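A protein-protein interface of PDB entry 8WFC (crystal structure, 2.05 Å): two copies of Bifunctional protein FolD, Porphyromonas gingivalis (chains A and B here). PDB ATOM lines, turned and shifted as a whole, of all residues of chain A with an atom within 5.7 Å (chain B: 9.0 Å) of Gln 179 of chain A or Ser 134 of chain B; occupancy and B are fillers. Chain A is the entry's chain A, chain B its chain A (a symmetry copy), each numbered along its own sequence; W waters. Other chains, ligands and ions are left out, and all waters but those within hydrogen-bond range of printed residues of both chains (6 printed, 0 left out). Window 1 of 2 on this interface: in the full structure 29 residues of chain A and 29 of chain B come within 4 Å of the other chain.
The side-chain amide oxygen (OD1) of Asn 171 of chain B lies close to the backbone carbonyl oxygen (O) of Ser 134 of chain A (3.5 Å). O of Ser 134 of chain A lies within hydrogen-bond range of NZ of Lys 175 of chain B (2.8 Å). The side-chain hydroxyl (OG) of Ser 134 of chain A is in hydrogen-bond range of the side-chain amide nitrogen (NE2) of Gln 179 of chain B (3.2 Å). OD1 of Asn 171 of chain A sits close to O of Ser 134 of chain B (3.5 Å). ND2 of Asn 171 of chain A is in hydrogen-bond range of O of Ile 135 of chain B, 3.1 Å away. The side-chain amino group (NZ) of Lys 175 of chain A is in hydrogen-bond range of the backbone carbonyl oxygen (O) of Ser 134 of chain B, at 2.8 Å. The side-chain amide nitrogen (NE2) of Gln 179 of chain A is in hydrogen-bond range of the side-chain hydroxyl (OG) of Ser 134 of chain B (3.2 Å). The backbone carbonyl oxygen (O) of Leu 182 of chain A lies within hydrogen-bond range of the guanidinium group (NH1) of Arg 169 of chain B (2.9 Å).
OD1 of Asn 171 of chain A is in hydrogen-bond range of NZ of Lys 175 of chain A (3.2 Å). The side-chain amide oxygen of Asn 171 of chain B sits at hydrogen-bond distance from the side-chain amino group of Lys 175 of chain B (3.2 Å).
Gly 131 of chain B touches Val 130 of chain A (CA to CG1, 3.9 Å). Ile 135 of chain B touches Val 130 of chain A (CD1 to CG2, 3.9 Å). Ile 194 of chain B touches Leu 182 of chain A (CD1 to CD2, 3.8 Å). O of Gln 183 of chain A touches NH1 of Arg 169 of chain B, 3.8 Å away.
Printed residues of chain B within 4 Å of Val 130 of chain A: Gly 131 (3.9 Å) and Ile 135 (3.9 Å). Of the printed residues of chain B, Gln 179 of chain A touches Ser 134. Pro 127 of chain B touches none of the printed residues of chain A. Of chain A, only Asn 171 (3.5 Å), Lys 175 (2.8 Å) and Gln 179 (3.2 Å) come within 4 Å of Ser 134 of chain B. Of the printed residues of chain A, Arg 169 of chain B touches Leu 182 (2.9 Å) and Gln 183 (3.8 Å). Of the printed residues of chain A, Asn 171 of chain B touches Ser 134 (3.5 Å). The nearest printed residue of chain B that does not touch Gln 179 of chain A is Gln 179 of chain B (4.01 Å). The nearest residue of chain A that does not touch Ser 134 of chain B is Val 130 of chain A (4.03 Å).
Of the 25 printed residues of chain B, 8 touch a printed residue of chain A. Of the 14 printed residues of chain A, 7 touch a printed residue of chain B. Along chain A the printed residues that touch a printed residue of chain B span positions 130 to 183. Among the printed residues, no Asp or Glu carboxylate lies within 4 Å of a Lys or Arg side-chain nitrogen of the other chain.
Ser 134 of chain A touches Asn 171 of chain B, and with the chains exchanged Asn 171 of chain A touches Ser 134 of chain B. Ser 134 of chain A touches Lys 175 of chain B, and with the chains exchanged Lys 175 of chain A touches Ser 134 of chain B. Ser 134 of chain A touches Gln 179 of chain B, and with the chains exchanged Gln 179 of chain A touches Ser 134 of chain B. Positions printed for both chains: 130, 133, 134, 171, 175, 176, 178, 179, 180, 182 and 183.
Water W6 lies within hydrogen-bond range of the side-chain hydroxyl of Ser 134 of chain A (2.7 Å) and the side-chain amide oxygen of Asn 171 of chain B (3.0 Å). Water W3 lies within hydrogen-bond range of the backbone carbonyl oxygen (O) of Gln 179 of chain B and the side-chain amino group (NZ) of Lys 175 of chain A. Water W2 lies within hydrogen-bond range of the side-chain amino group of Lys 175 of chain A and the backbone carbonyl oxygen of Leu 182 of chain B.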
ATOM      1  N   VAL A 130      17.407  21.361  22.554  1.00  0.00           N
ATOM      2  CA  VAL A 130      16.565  21.900  21.485  1.00  0.00           C
ATOM      3  C   VAL A 130      15.252  22.410  22.059  1.00  0.00           C
ATOM      4  O   VAL A 130      14.772  23.483  21.679  1.00  0.00           O
ATOM      5  CB  VAL A 130      16.334  20.840  20.391  1.00  0.00           C
ATOM      6  CG1 VAL A 130      15.279  21.318  19.388  1.00  0.00           C
ATOM      7  CG2 VAL A 130      17.655  20.529  19.674  1.00  0.00           C
ATOM      8  N   LEU A 133      15.739  25.600  24.222  1.00  0.00           N
ATOM      9  CA  LEU A 133      15.883  26.756  23.341  1.00  0.00           C
ATOM     10  C   LEU A 133      14.511  27.288  22.912  1.00  0.00           C
ATOM     11  O   LEU A 133      14.241  28.486  23.019  1.00  0.00           O
ATOM     12  CB  LEU A 133      16.740  26.379  22.123  1.00  0.00           C
ATOM     13  CG  LEU A 133      16.844  27.370  20.945  1.00  0.00           C
ATOM     14  CD1 LEU A 133      17.202  28.720  21.480  1.00  0.00           C
ATOM     15  CD2 LEU A 133      17.906  26.940  19.917  1.00  0.00           C
ATOM     16  N   SER A 134      13.631  26.407  22.425  1.00  0.00           N
ATOM     17  CA  SER A 134      12.302  26.856  22.001  1.00  0.00           C
ATOM     18  C   SER A 134      11.531  27.516  23.140  1.00  0.00           C
ATOM     19  O   SER A 134      10.847  28.528  22.936  1.00  0.00           O
ATOM     20  CB  SER A 134      11.498  25.686  21.446  1.00  0.00           C
ATOM     21  OG  SER A 134      10.291  26.152  20.884  1.00  0.00           O
ATOM     22  N   ASN A 171      17.006  21.325  10.602  1.00  0.00           N
ATOM     23  CA  ASN A 171      17.196  21.230  12.065  1.00  0.00           C
ATOM     24  C   ASN A 171      18.518  21.899  12.422  1.00  0.00           C
ATOM     25  O   ASN A 171      18.612  22.461  13.472  1.00  0.00           O
ATOM     26  CB  ASN A 171      17.227  19.777  12.515  1.00  0.00           C
ATOM     27  CG  ASN A 171      15.844  19.185  12.615  1.00  0.00           C
ATOM     28  OD1 ASN A 171      14.908  19.885  12.926  1.00  0.00           O
ATOM     29  ND2 ASN A 171      15.715  17.908  12.342  1.00  0.00           N
ATOM     30  N   GLY A 174      17.758  26.364  10.027  1.00  0.00           N
ATOM     31  CA  GLY A 174      16.550  27.164   9.824  1.00  0.00           C
ATOM     32  C   GLY A 174      15.673  27.241  11.062  1.00  0.00           C
ATOM     33  O   GLY A 174      15.275  28.330  11.500  1.00  0.00           O
ATOM     34  N   LYS A 175      15.371  26.085  11.652  1.00  0.00           N
ATOM     35  CA  LYS A 175      14.525  26.074  12.843  1.00  0.00           C
ATOM     36  C   LYS A 175      15.175  26.765  14.030  1.00  0.00           C
ATOM     37  O   LYS A 175      14.527  27.640  14.625  1.00  0.00           O
ATOM     38  CB  LYS A 175      14.101  24.638  13.178  1.00  0.00           C
ATOM     39  CG  LYS A 175      13.196  23.994  12.120  1.00  0.00           C
ATOM     40  CD  LYS A 175      13.077  22.492  12.367  1.00  0.00           C
ATOM     41  CE  LYS A 175      11.913  21.858  11.609  1.00  0.00           C
ATOM     42  NZ  LYS A 175      12.019  20.366  11.686  1.00  0.00           N
ATOM     43  N   PRO A 176      16.418  26.451  14.434  1.00  0.00           N
ATOM     44  CA  PRO A 176      16.966  27.146  15.614  1.00  0.00           C
ATOM     45  C   PRO A 176      17.209  28.635  15.405  1.00  0.00           C
ATOM     46  O   PRO A 176      16.994  29.411  16.344  1.00  0.00           O
ATOM     47  CB  PRO A 176      18.279  26.388  15.903  1.00  0.00           C
ATOM     48  CG  PRO A 176      18.630  25.715  14.618  1.00  0.00           C
ATOM     49  CD  PRO A 176      17.301  25.350  13.998  1.00  0.00           C
ATOM     50  N   VAL A 177      17.683  29.069  14.231  1.00  0.00           N
ATOM     51  CA  VAL A 177      17.873  30.509  14.040  1.00  0.00           C
ATOM     52  C   VAL A 177      16.532  31.234  14.139  1.00  0.00           C
ATOM     53  O   VAL A 177      16.432  32.303  14.754  1.00  0.00           O
ATOM     54  CB  VAL A 177      18.592  30.822  12.711  1.00  0.00           C
ATOM     55  CG1 VAL A 177      17.712  30.545  11.529  1.00  0.00           C
ATOM     56  CG2 VAL A 177      18.953  32.305  12.651  1.00  0.00           C
ATOM     57  N   SER A 178      15.475  30.638  13.581  1.00  0.00           N
ATOM     58  CA  SER A 178      14.139  31.211  13.708  1.00  0.00           C
ATOM     59  C   SER A 178      13.748  31.351  15.168  1.00  0.00           C
ATOM     60  O   SER A 178      13.191  32.374  15.573  1.00  0.00           O
ATOM     61  CB  SER A 178      13.128  30.340  12.965  1.00  0.00           C
ATOM     62  OG  SER A 178      13.377  30.432  11.584  1.00  0.00           O
ATOM     63  N   GLN A 179      14.048  30.336  15.982  1.00  0.00           N
ATOM     64  CA  GLN A 179      13.664  30.389  17.387  1.00  0.00           C
ATOM     65  C   GLN A 179      14.450  31.454  18.141  1.00  0.00           C
ATOM     66  O   GLN A 179      13.883  32.177  18.964  1.00  0.00           O
ATOM     67  CB  GLN A 179      13.841  29.004  18.017  1.00  0.00           C
ATOM     68  CG  GLN A 179      12.860  28.002  17.388  1.00  0.00           C
ATOM     69  CD  GLN A 179      13.107  26.560  17.799  1.00  0.00           C
ATOM     70  OE1 GLN A 179      13.622  26.291  18.884  1.00  0.00           O
ATOM     71  NE2 GLN A 179      12.712  25.622  16.935  1.00  0.00           N
ATOM     72  N   LEU A 180      15.744  31.591  17.848  1.00  0.00           N
ATOM     73  CA  LEU A 180      16.550  32.615  18.503  1.00  0.00           C
ATOM     74  C   LEU A 180      16.062  34.019  18.156  1.00  0.00           C
ATOM     75  O   LEU A 180      15.947  34.876  19.039  1.00  0.00           O
ATOM     76  CB  LEU A 180      18.023  32.454  18.109  1.00  0.00           C
ATOM     77  CG  LEU A 180      18.735  31.233  18.696  1.00  0.00           C
ATOM     78  CD1 LEU A 180      20.054  30.991  18.002  1.00  0.00           C
ATOM     79  CD2 LEU A 180      18.947  31.427  20.186  1.00  0.00           C
ATOM     80  N   LEU A 181      15.775  34.279  16.889  1.00  0.00           N
ATOM     81  CA  LEU A 181      15.392  35.628  16.479  1.00  0.00           C
ATOM     82  C   LEU A 181      13.926  35.939  16.759  1.00  0.00           C
ATOM     83  O   LEU A 181      13.494  37.083  16.557  1.00  0.00           O
ATOM     84  CB  LEU A 181      15.731  35.826  15.002  1.00  0.00           C
ATOM     85  CG  LEU A 181      17.253  35.880  14.773  1.00  0.00           C
ATOM     86  CD1 LEU A 181      17.583  35.936  13.300  1.00  0.00           C
ATOM     87  CD2 LEU A 181      17.898  37.050  15.517  1.00  0.00           C
ATOM     88  N   LEU A 182      13.161  34.961  17.236  1.00  0.00           N
ATOM     89  CA  LEU A 182      11.817  35.188  17.754  1.00  0.00           C
ATOM     90  C   LEU A 182      11.816  35.492  19.245  1.00  0.00           C
ATOM     91  O   LEU A 182      10.769  35.841  19.798  1.00  0.00           O
ATOM     92  CB  LEU A 182      10.936  33.957  17.478  1.00  0.00           C
ATOM     93  CG  LEU A 182       9.415  34.020  17.469  1.00  0.00           C
ATOM     94  CD1 LEU A 182       8.888  34.979  16.409  1.00  0.00           C
ATOM     95  CD2 LEU A 182       8.931  32.598  17.203  1.00  0.00           C
ATOM     96  N   GLN A 183      12.951  35.358  19.914  1.00  0.00           N
ATOM     97  CA  GLN A 183      13.014  35.693  21.324  1.00  0.00           C
ATOM     98  C   GLN A 183      12.855  37.195  21.524  1.00  0.00           C
ATOM     99  O   GLN A 183      13.104  37.993  20.627  1.00  0.00           O
ATOM    100  CB  GLN A 183      14.335  35.214  21.919  1.00  0.00           C
ATOM    101  CG  GLN A 183      14.386  33.692  22.053  1.00  0.00           C
ATOM    102  CD  GLN A 183      15.706  33.194  22.578  1.00  0.00           C
ATOM    103  OE1 GLN A 183      16.692  33.940  22.611  1.00  0.00           O
ATOM    104  NE2 GLN A 183      15.740  31.928  23.010  1.00  0.00           N
ATOM    105  N   PRO B 127      10.672  19.497  28.278  1.00  0.00           N
ATOM    106  CA  PRO B 127      11.491  20.073  27.194  1.00  0.00           C
ATOM    107  C   PRO B 127      12.006  19.040  26.201  1.00  0.00           C
ATOM    108  O   PRO B 127      12.247  19.380  25.035  1.00  0.00           O
ATOM    109  CB  PRO B 127      12.634  20.765  27.954  1.00  0.00           C
ATOM    110  CG  PRO B 127      12.016  21.145  29.275  1.00  0.00           C
ATOM    111  CD  PRO B 127      11.048  20.012  29.609  1.00  0.00           C
ATOM    112  N   ILE B 128      12.159  17.777  26.608  1.00  0.00           N
ATOM    113  CA  ILE B 128      12.612  16.782  25.639  1.00  0.00           C
ATOM    114  C   ILE B 128      11.517  16.483  24.618  1.00  0.00           C
ATOM    115  O   ILE B 128      11.812  16.181  23.453  1.00  0.00           O
ATOM    116  CB  ILE B 128      13.107  15.509  26.347  1.00  0.00           C
ATOM    117  CG1 ILE B 128      14.145  14.784  25.479  1.00  0.00           C
ATOM    118  CG2 ILE B 128      11.946  14.567  26.666  1.00  0.00           C
ATOM    119  CD1 ILE B 128      14.742  13.554  26.151  1.00  0.00           C
ATOM    120  N   ASN B 129      10.246  16.565  25.015  1.00  0.00           N
ATOM    121  CA  ASN B 129       9.187  16.367  24.036  1.00  0.00           C
ATOM    122  C   ASN B 129       9.022  17.605  23.165  1.00  0.00           C
ATOM    123  O   ASN B 129       8.778  17.492  21.954  1.00  0.00           O
ATOM    124  CB  ASN B 129       7.877  16.007  24.740  1.00  0.00           C
ATOM    125  CG  ASN B 129       7.812  14.544  25.116  1.00  0.00           C
ATOM    126  OD1 ASN B 129       8.307  13.688  24.385  1.00  0.00           O
ATOM    127  ND2 ASN B 129       7.209  14.244  26.262  1.00  0.00           N
ATOM    128  N   VAL B 130       9.180  18.793  23.758  1.00  0.00           N
ATOM    129  CA  VAL B 130       9.198  20.020  22.961  1.00  0.00           C
ATOM    130  C   VAL B 130      10.305  19.952  21.919  1.00  0.00           C
ATOM    131  O   VAL B 130      10.105  20.333  20.761  1.00  0.00           O
ATOM    132  CB  VAL B 130       9.347  21.255  23.869  1.00  0.00           C
ATOM    133  CG1 VAL B 130       9.591  22.516  23.034  1.00  0.00           C
ATOM    134  CG2 VAL B 130       8.094  21.421  24.740  1.00  0.00           C
ATOM    135  N   GLY B 131      11.481  19.446  22.307  1.00  0.00           N
ATOM    136  CA  GLY B 131      12.582  19.355  21.359  1.00  0.00           C
ATOM    137  C   GLY B 131      12.367  18.273  20.318  1.00  0.00           C
ATOM    138  O   GLY B 131      12.660  18.472  19.131  1.00  0.00           O
ATOM    139  N   ARG B 132      11.854  17.110  20.744  1.00  0.00           N
ATOM    140  CA  ARG B 132      11.525  16.061  19.785  1.00  0.00           C
ATOM    141  C   ARG B 132      10.551  16.573  18.725  1.00  0.00           C
ATOM    142  O   ARG B 132      10.688  16.263  17.536  1.00  0.00           O
ATOM    143  CB  ARG B 132      10.905  14.876  20.518  1.00  0.00           C
ATOM    144  CG  ARG B 132      11.879  13.879  21.110  1.00  0.00           C
ATOM    145  CD  ARG B 132      11.298  13.303  22.407  1.00  0.00           C
ATOM    146  NE  ARG B 132      12.189  12.318  23.014  1.00  0.00           N
ATOM    147  CZ  ARG B 132      11.775  11.408  23.889  1.00  0.00           C
ATOM    148  NH1 ARG B 132      10.501  11.410  24.280  1.00  0.00           N
ATOM    149  NH2 ARG B 132      12.625  10.506  24.382  1.00  0.00           N
ATOM    150  N   LEU B 133       9.547  17.340  19.145  1.00  0.00           N
ATOM    151  CA  LEU B 133       8.596  17.915  18.197  1.00  0.00           C
ATOM    152  C   LEU B 133       9.317  18.774  17.154  1.00  0.00           C
ATOM    153  O   LEU B 133       9.103  18.613  15.950  1.00  0.00           O
ATOM    154  CB  LEU B 133       7.535  18.728  18.953  1.00  0.00           C
ATOM    155  CG  LEU B 133       6.556  19.611  18.149  1.00  0.00           C
ATOM    156  CD1 LEU B 133       5.951  18.789  17.057  1.00  0.00           C
ATOM    157  CD2 LEU B 133       5.429  20.178  19.032  1.00  0.00           C
ATOM    158  N   SER B 134      10.180  19.694  17.600  1.00  0.00           N
ATOM    159  CA  SER B 134      10.902  20.544  16.650  1.00  0.00           C
ATOM    160  C   SER B 134      11.746  19.726  15.678  1.00  0.00           C
ATOM    161  O   SER B 134      11.812  20.039  14.482  1.00  0.00           O
ATOM    162  CB  SER B 134      11.789  21.536  17.393  1.00  0.00           C
ATOM    163  OG  SER B 134      12.347  22.461  16.485  1.00  0.00           O
ATOM    164  N   ILE B 135      12.438  18.706  16.186  1.00  0.00           N
ATOM    165  CA  ILE B 135      13.352  17.930  15.351  1.00  0.00           C
ATOM    166  C   ILE B 135      12.584  17.027  14.390  1.00  0.00           C
ATOM    167  O   ILE B 135      13.050  16.745  13.276  1.00  0.00           O
ATOM    168  CB  ILE B 135      14.314  17.113  16.240  1.00  0.00           C
ATOM    169  CG1 ILE B 135      15.207  18.035  17.077  1.00  0.00           C
ATOM    170  CG2 ILE B 135      15.155  16.136  15.412  1.00  0.00           C
ATOM    171  CD1 ILE B 135      15.692  17.380  18.369  1.00  0.00           C
ATOM    172  N   GLY B 136      11.407  16.570  14.785  1.00  0.00           N
ATOM    173  CA  GLY B 136      10.687  15.566  14.036  1.00  0.00           C
ATOM    174  C   GLY B 136      10.813  14.154  14.573  1.00  0.00           C
ATOM    175  O   GLY B 136      10.671  13.206  13.799  1.00  0.00           O
ATOM    176  N   LEU B 137      11.080  13.983  15.867  1.00  0.00           N
ATOM    177  CA  LEU B 137      11.163  12.667  16.485  1.00  0.00           C
ATOM    178  C   LEU B 137       9.869  12.359  17.235  1.00  0.00           C
ATOM    179  O   LEU B 137       9.161  13.276  17.652  1.00  0.00           O
ATOM    180  CB  LEU B 137      12.342  12.605  17.464  1.00  0.00           C
ATOM    181  CG  LEU B 137      13.705  13.014  16.918  1.00  0.00           C
ATOM    182  CD1 LEU B 137      14.669  13.319  18.068  1.00  0.00           C
ATOM    183  CD2 LEU B 137      14.248  11.903  16.019  1.00  0.00           C
ATOM    184  N   PRO B 138       9.511  11.086  17.428  1.00  0.00           N
ATOM    185  CA  PRO B 138       8.300  10.780  18.201  1.00  0.00           C
ATOM    186  C   PRO B 138       8.387  11.325  19.623  1.00  0.00           C
ATOM    187  O   PRO B 138       9.433  11.267  20.273  1.00  0.00           O
ATOM    188  CB  PRO B 138       8.239   9.243  18.185  1.00  0.00           C
ATOM    189  CG  PRO B 138       9.112   8.827  17.043  1.00  0.00           C
ATOM    190  CD  PRO B 138      10.199   9.869  16.973  1.00  0.00           C
ATOM    191  N   GLY B 139       7.269  11.868  20.088  1.00  0.00           N
ATOM    192  CA  GLY B 139       7.143  12.369  21.449  1.00  0.00           C
ATOM    193  C   GLY B 139       5.754  12.945  21.591  1.00  0.00           C
ATOM    194  O   GLY B 139       5.027  13.118  20.609  1.00  0.00           O
ATOM    195  N   PHE B 140       5.383  13.253  22.827  1.00  0.00           N
ATOM    196  CA  PHE B 140       4.046  13.788  23.034  1.00  0.00           C
ATOM    197  C   PHE B 140       3.974  15.227  22.542  1.00  0.00           C
ATOM    198  O   PHE B 140       4.838  16.053  22.858  1.00  0.00           O
ATOM    199  CB  PHE B 140       3.639  13.698  24.506  1.00  0.00           C
ATOM    200  CG  PHE B 140       3.285  12.297  24.943  1.00  0.00           C
ATOM    201  CD1 PHE B 140       2.246  11.616  24.332  1.00  0.00           C
ATOM    202  CD2 PHE B 140       3.994  11.662  25.946  1.00  0.00           C
ATOM    203  CE1 PHE B 140       1.914  10.327  24.715  1.00  0.00           C
ATOM    204  CE2 PHE B 140       3.660  10.373  26.337  1.00  0.00           C
ATOM    205  CZ  PHE B 140       2.624   9.706  25.714  1.00  0.00           C
ATOM    206  N   VAL B 141       2.965  15.506  21.726  1.00  0.00           N
ATOM    207  CA  VAL B 141       2.656  16.857  21.292  1.00  0.00           C
ATOM    208  C   VAL B 141       1.678  17.453  22.293  1.00  0.00           C
ATOM    209  O   VAL B 141       0.693  16.801  22.658  1.00  0.00           O
ATOM    210  CB  VAL B 141       2.058  16.853  19.874  1.00  0.00           C
ATOM    211  CG1 VAL B 141       1.730  18.279  19.446  1.00  0.00           C
ATOM    212  CG2 VAL B 141       3.019  16.183  18.900  1.00  0.00           C
ATOM    213  N   ARG B 169       3.529  34.260  19.803  1.00  0.00           N
ATOM    214  CA  ARG B 169       4.705  33.411  19.887  1.00  0.00           C
ATOM    215  C   ARG B 169       4.731  32.668  21.216  1.00  0.00           C
ATOM    216  O   ARG B 169       5.800  32.393  21.764  1.00  0.00           O
ATOM    217  CB  ARG B 169       5.979  34.235  19.692  1.00  0.00           C
ATOM    218  CG  ARG B 169       6.007  35.513  20.544  1.00  0.00           C
ATOM    219  CD  ARG B 169       7.395  36.181  20.608  1.00  0.00           C
ATOM    220  NE  ARG B 169       7.242  37.544  21.119  1.00  0.00           N
ATOM    221  CZ  ARG B 169       8.154  38.498  21.010  1.00  0.00           C
ATOM    222  NH1 ARG B 169       9.334  38.245  20.441  1.00  0.00           N
ATOM    223  NH2 ARG B 169       7.888  39.703  21.483  1.00  0.00           N
ATOM    224  N   ASN B 171       4.469  29.778  24.134  1.00  0.00           N
ATOM    225  CA  ASN B 171       4.970  28.391  24.237  1.00  0.00           C
ATOM    226  C   ASN B 171       3.779  27.443  24.175  1.00  0.00           C
ATOM    227  O   ASN B 171       3.921  26.374  23.661  1.00  0.00           O
ATOM    228  CB  ASN B 171       5.717  28.181  25.547  1.00  0.00           C
ATOM    229  CG  ASN B 171       7.120  28.728  25.493  1.00  0.00           C
ATOM    230  OD1 ASN B 171       7.733  28.720  24.451  1.00  0.00           O
ATOM    231  ND2 ASN B 171       7.620  29.210  26.607  1.00  0.00           N
ATOM    232  N   LYS B 175       4.339  28.797  19.088  1.00  0.00           N
ATOM    233  CA  LYS B 175       5.535  28.058  18.690  1.00  0.00           C
ATOM    234  C   LYS B 175       5.232  26.624  18.288  1.00  0.00           C
ATOM    235  O   LYS B 175       5.661  26.220  17.197  1.00  0.00           O
ATOM    236  CB  LYS B 175       6.595  28.131  19.796  1.00  0.00           C
ATOM    237  CG  LYS B 175       7.142  29.543  20.041  1.00  0.00           C
ATOM    238  CD  LYS B 175       7.943  29.583  21.341  1.00  0.00           C
ATOM    239  CE  LYS B 175       8.824  30.826  21.455  1.00  0.00           C
ATOM    240  NZ  LYS B 175       9.367  30.928  22.847  1.00  0.00           N
ATOM    241  N   PRO B 176       4.517  25.807  19.081  1.00  0.00           N
ATOM    242  CA  PRO B 176       4.292  24.420  18.633  1.00  0.00           C
ATOM    243  C   PRO B 176       3.411  24.298  17.397  1.00  0.00           C
ATOM    244  O   PRO B 176       3.673  23.422  16.562  1.00  0.00           O
ATOM    245  CB  PRO B 176       3.651  23.742  19.862  1.00  0.00           C
ATOM    246  CG  PRO B 176       3.090  24.861  20.674  1.00  0.00           C
ATOM    247  CD  PRO B 176       4.055  26.007  20.470  1.00  0.00           C
ATOM    248  N   SER B 178       3.250  26.354  14.929  1.00  0.00           N
ATOM    249  CA  SER B 178       4.161  26.691  13.840  1.00  0.00           C
ATOM    250  C   SER B 178       5.040  25.505  13.485  1.00  0.00           C
ATOM    251  O   SER B 178       5.255  25.214  12.306  1.00  0.00           O
ATOM    252  CB  SER B 178       5.017  27.893  14.232  1.00  0.00           C
ATOM    253  OG  SER B 178       4.195  29.030  14.314  1.00  0.00           O
ATOM    254  N   GLN B 179       5.546  24.794  14.496  1.00  0.00           N
ATOM    255  CA  GLN B 179       6.431  23.668  14.226  1.00  0.00           C
ATOM    256  C   GLN B 179       5.685  22.518  13.561  1.00  0.00           C
ATOM    257  O   GLN B 179       6.204  21.896  12.631  1.00  0.00           O
ATOM    258  CB  GLN B 179       7.108  23.226  15.527  1.00  0.00           C
ATOM    259  CG  GLN B 179       8.040  24.332  16.046  1.00  0.00           C
ATOM    260  CD  GLN B 179       8.589  24.068  17.438  1.00  0.00           C
ATOM    261  OE1 GLN B 179       8.737  22.920  17.853  1.00  0.00           O
ATOM    262  NE2 GLN B 179       8.920  25.143  18.157  1.00  0.00           N
ATOM    263  N   LEU B 180       4.453  22.246  13.996  1.00  0.00           N
ATOM    264  CA  LEU B 180       3.666  21.184  13.382  1.00  0.00           C
ATOM    265  C   LEU B 180       3.355  21.491  11.919  1.00  0.00           C
ATOM    266  O   LEU B 180       3.479  20.615  11.057  1.00  0.00           O
ATOM    267  CB  LEU B 180       2.366  20.975  14.167  1.00  0.00           C
ATOM    268  CG  LEU B 180       2.523  20.334  15.548  1.00  0.00           C
ATOM    269  CD1 LEU B 180       1.254  20.471  16.355  1.00  0.00           C
ATOM    270  CD2 LEU B 180       2.903  18.873  15.399  1.00  0.00           C
ATOM    271  N   LEU B 182       4.948  23.348   9.880  1.00  0.00           N
ATOM    272  CA  LEU B 182       6.170  23.384   9.084  1.00  0.00           C
ATOM    273  C   LEU B 182       6.679  21.991   8.745  1.00  0.00           C
ATOM    274  O   LEU B 182       7.625  21.859   7.963  1.00  0.00           O
ATOM    275  CB  LEU B 182       7.261  24.164   9.838  1.00  0.00           C
ATOM    276  CG  LEU B 182       8.469  24.770   9.139  1.00  0.00           C
ATOM    277  CD1 LEU B 182       8.067  25.802   8.093  1.00  0.00           C
ATOM    278  CD2 LEU B 182       9.320  25.409  10.233  1.00  0.00           C
ATOM    279  N   GLN B 183       6.093  20.951   9.318  1.00  0.00           N
ATOM    280  CA  GLN B 183       6.503  19.601   8.980  1.00  0.00           C
ATOM    281  C   GLN B 183       6.117  19.268   7.545  1.00  0.00           C
ATOM    282  O   GLN B 183       5.216  19.866   6.966  1.00  0.00           O
ATOM    283  CB  GLN B 183       5.872  18.604   9.947  1.00  0.00           C
ATOM    284  CG  GLN B 183       6.495  18.681  11.341  1.00  0.00           C
ATOM    285  CD  GLN B 183       5.843  17.749  12.327  1.00  0.00           C
ATOM    286  OE1 GLN B 183       4.757  17.218  12.066  1.00  0.00           O
ATOM    287  NE2 GLN B 183       6.504  17.527  13.468  1.00  0.00           N
ATOM    288  N   ILE B 194       5.302  34.054  11.810  1.00  0.00           N
ATOM    289  CA  ILE B 194       4.921  34.224  13.212  1.00  0.00           C
ATOM    290  C   ILE B 194       5.009  35.701  13.550  1.00  0.00           C
ATOM    291  O   ILE B 194       6.073  36.313  13.398  1.00  0.00           O
ATOM    292  CB  ILE B 194       5.819  33.415  14.158  1.00  0.00           C
ATOM    293  CG1 ILE B 194       5.811  31.940  13.779  1.00  0.00           C
ATOM    294  CG2 ILE B 194       5.366  33.611  15.615  1.00  0.00           C
ATOM    295  CD1 ILE B 194       7.089  31.240  14.143  1.00  0.00           C
HETATM  296  O   HOH W   1      14.660  21.515  15.374  1.00  0.00           O
HETATM  297  O   HOH W   2      10.094  20.010   9.192  1.00  0.00           O
HETATM  298  O   HOH W   3       9.063  21.759  12.754  1.00  0.00           O
HETATM  299  O   HOH W   4      11.665  30.943  20.291  1.00  0.00           O
HETATM  300  O   HOH W   5      10.020  34.007  22.463  1.00  0.00           O
HETATM  301  O   HOH W   6       8.318  26.369  22.765  1.00  0.00           O
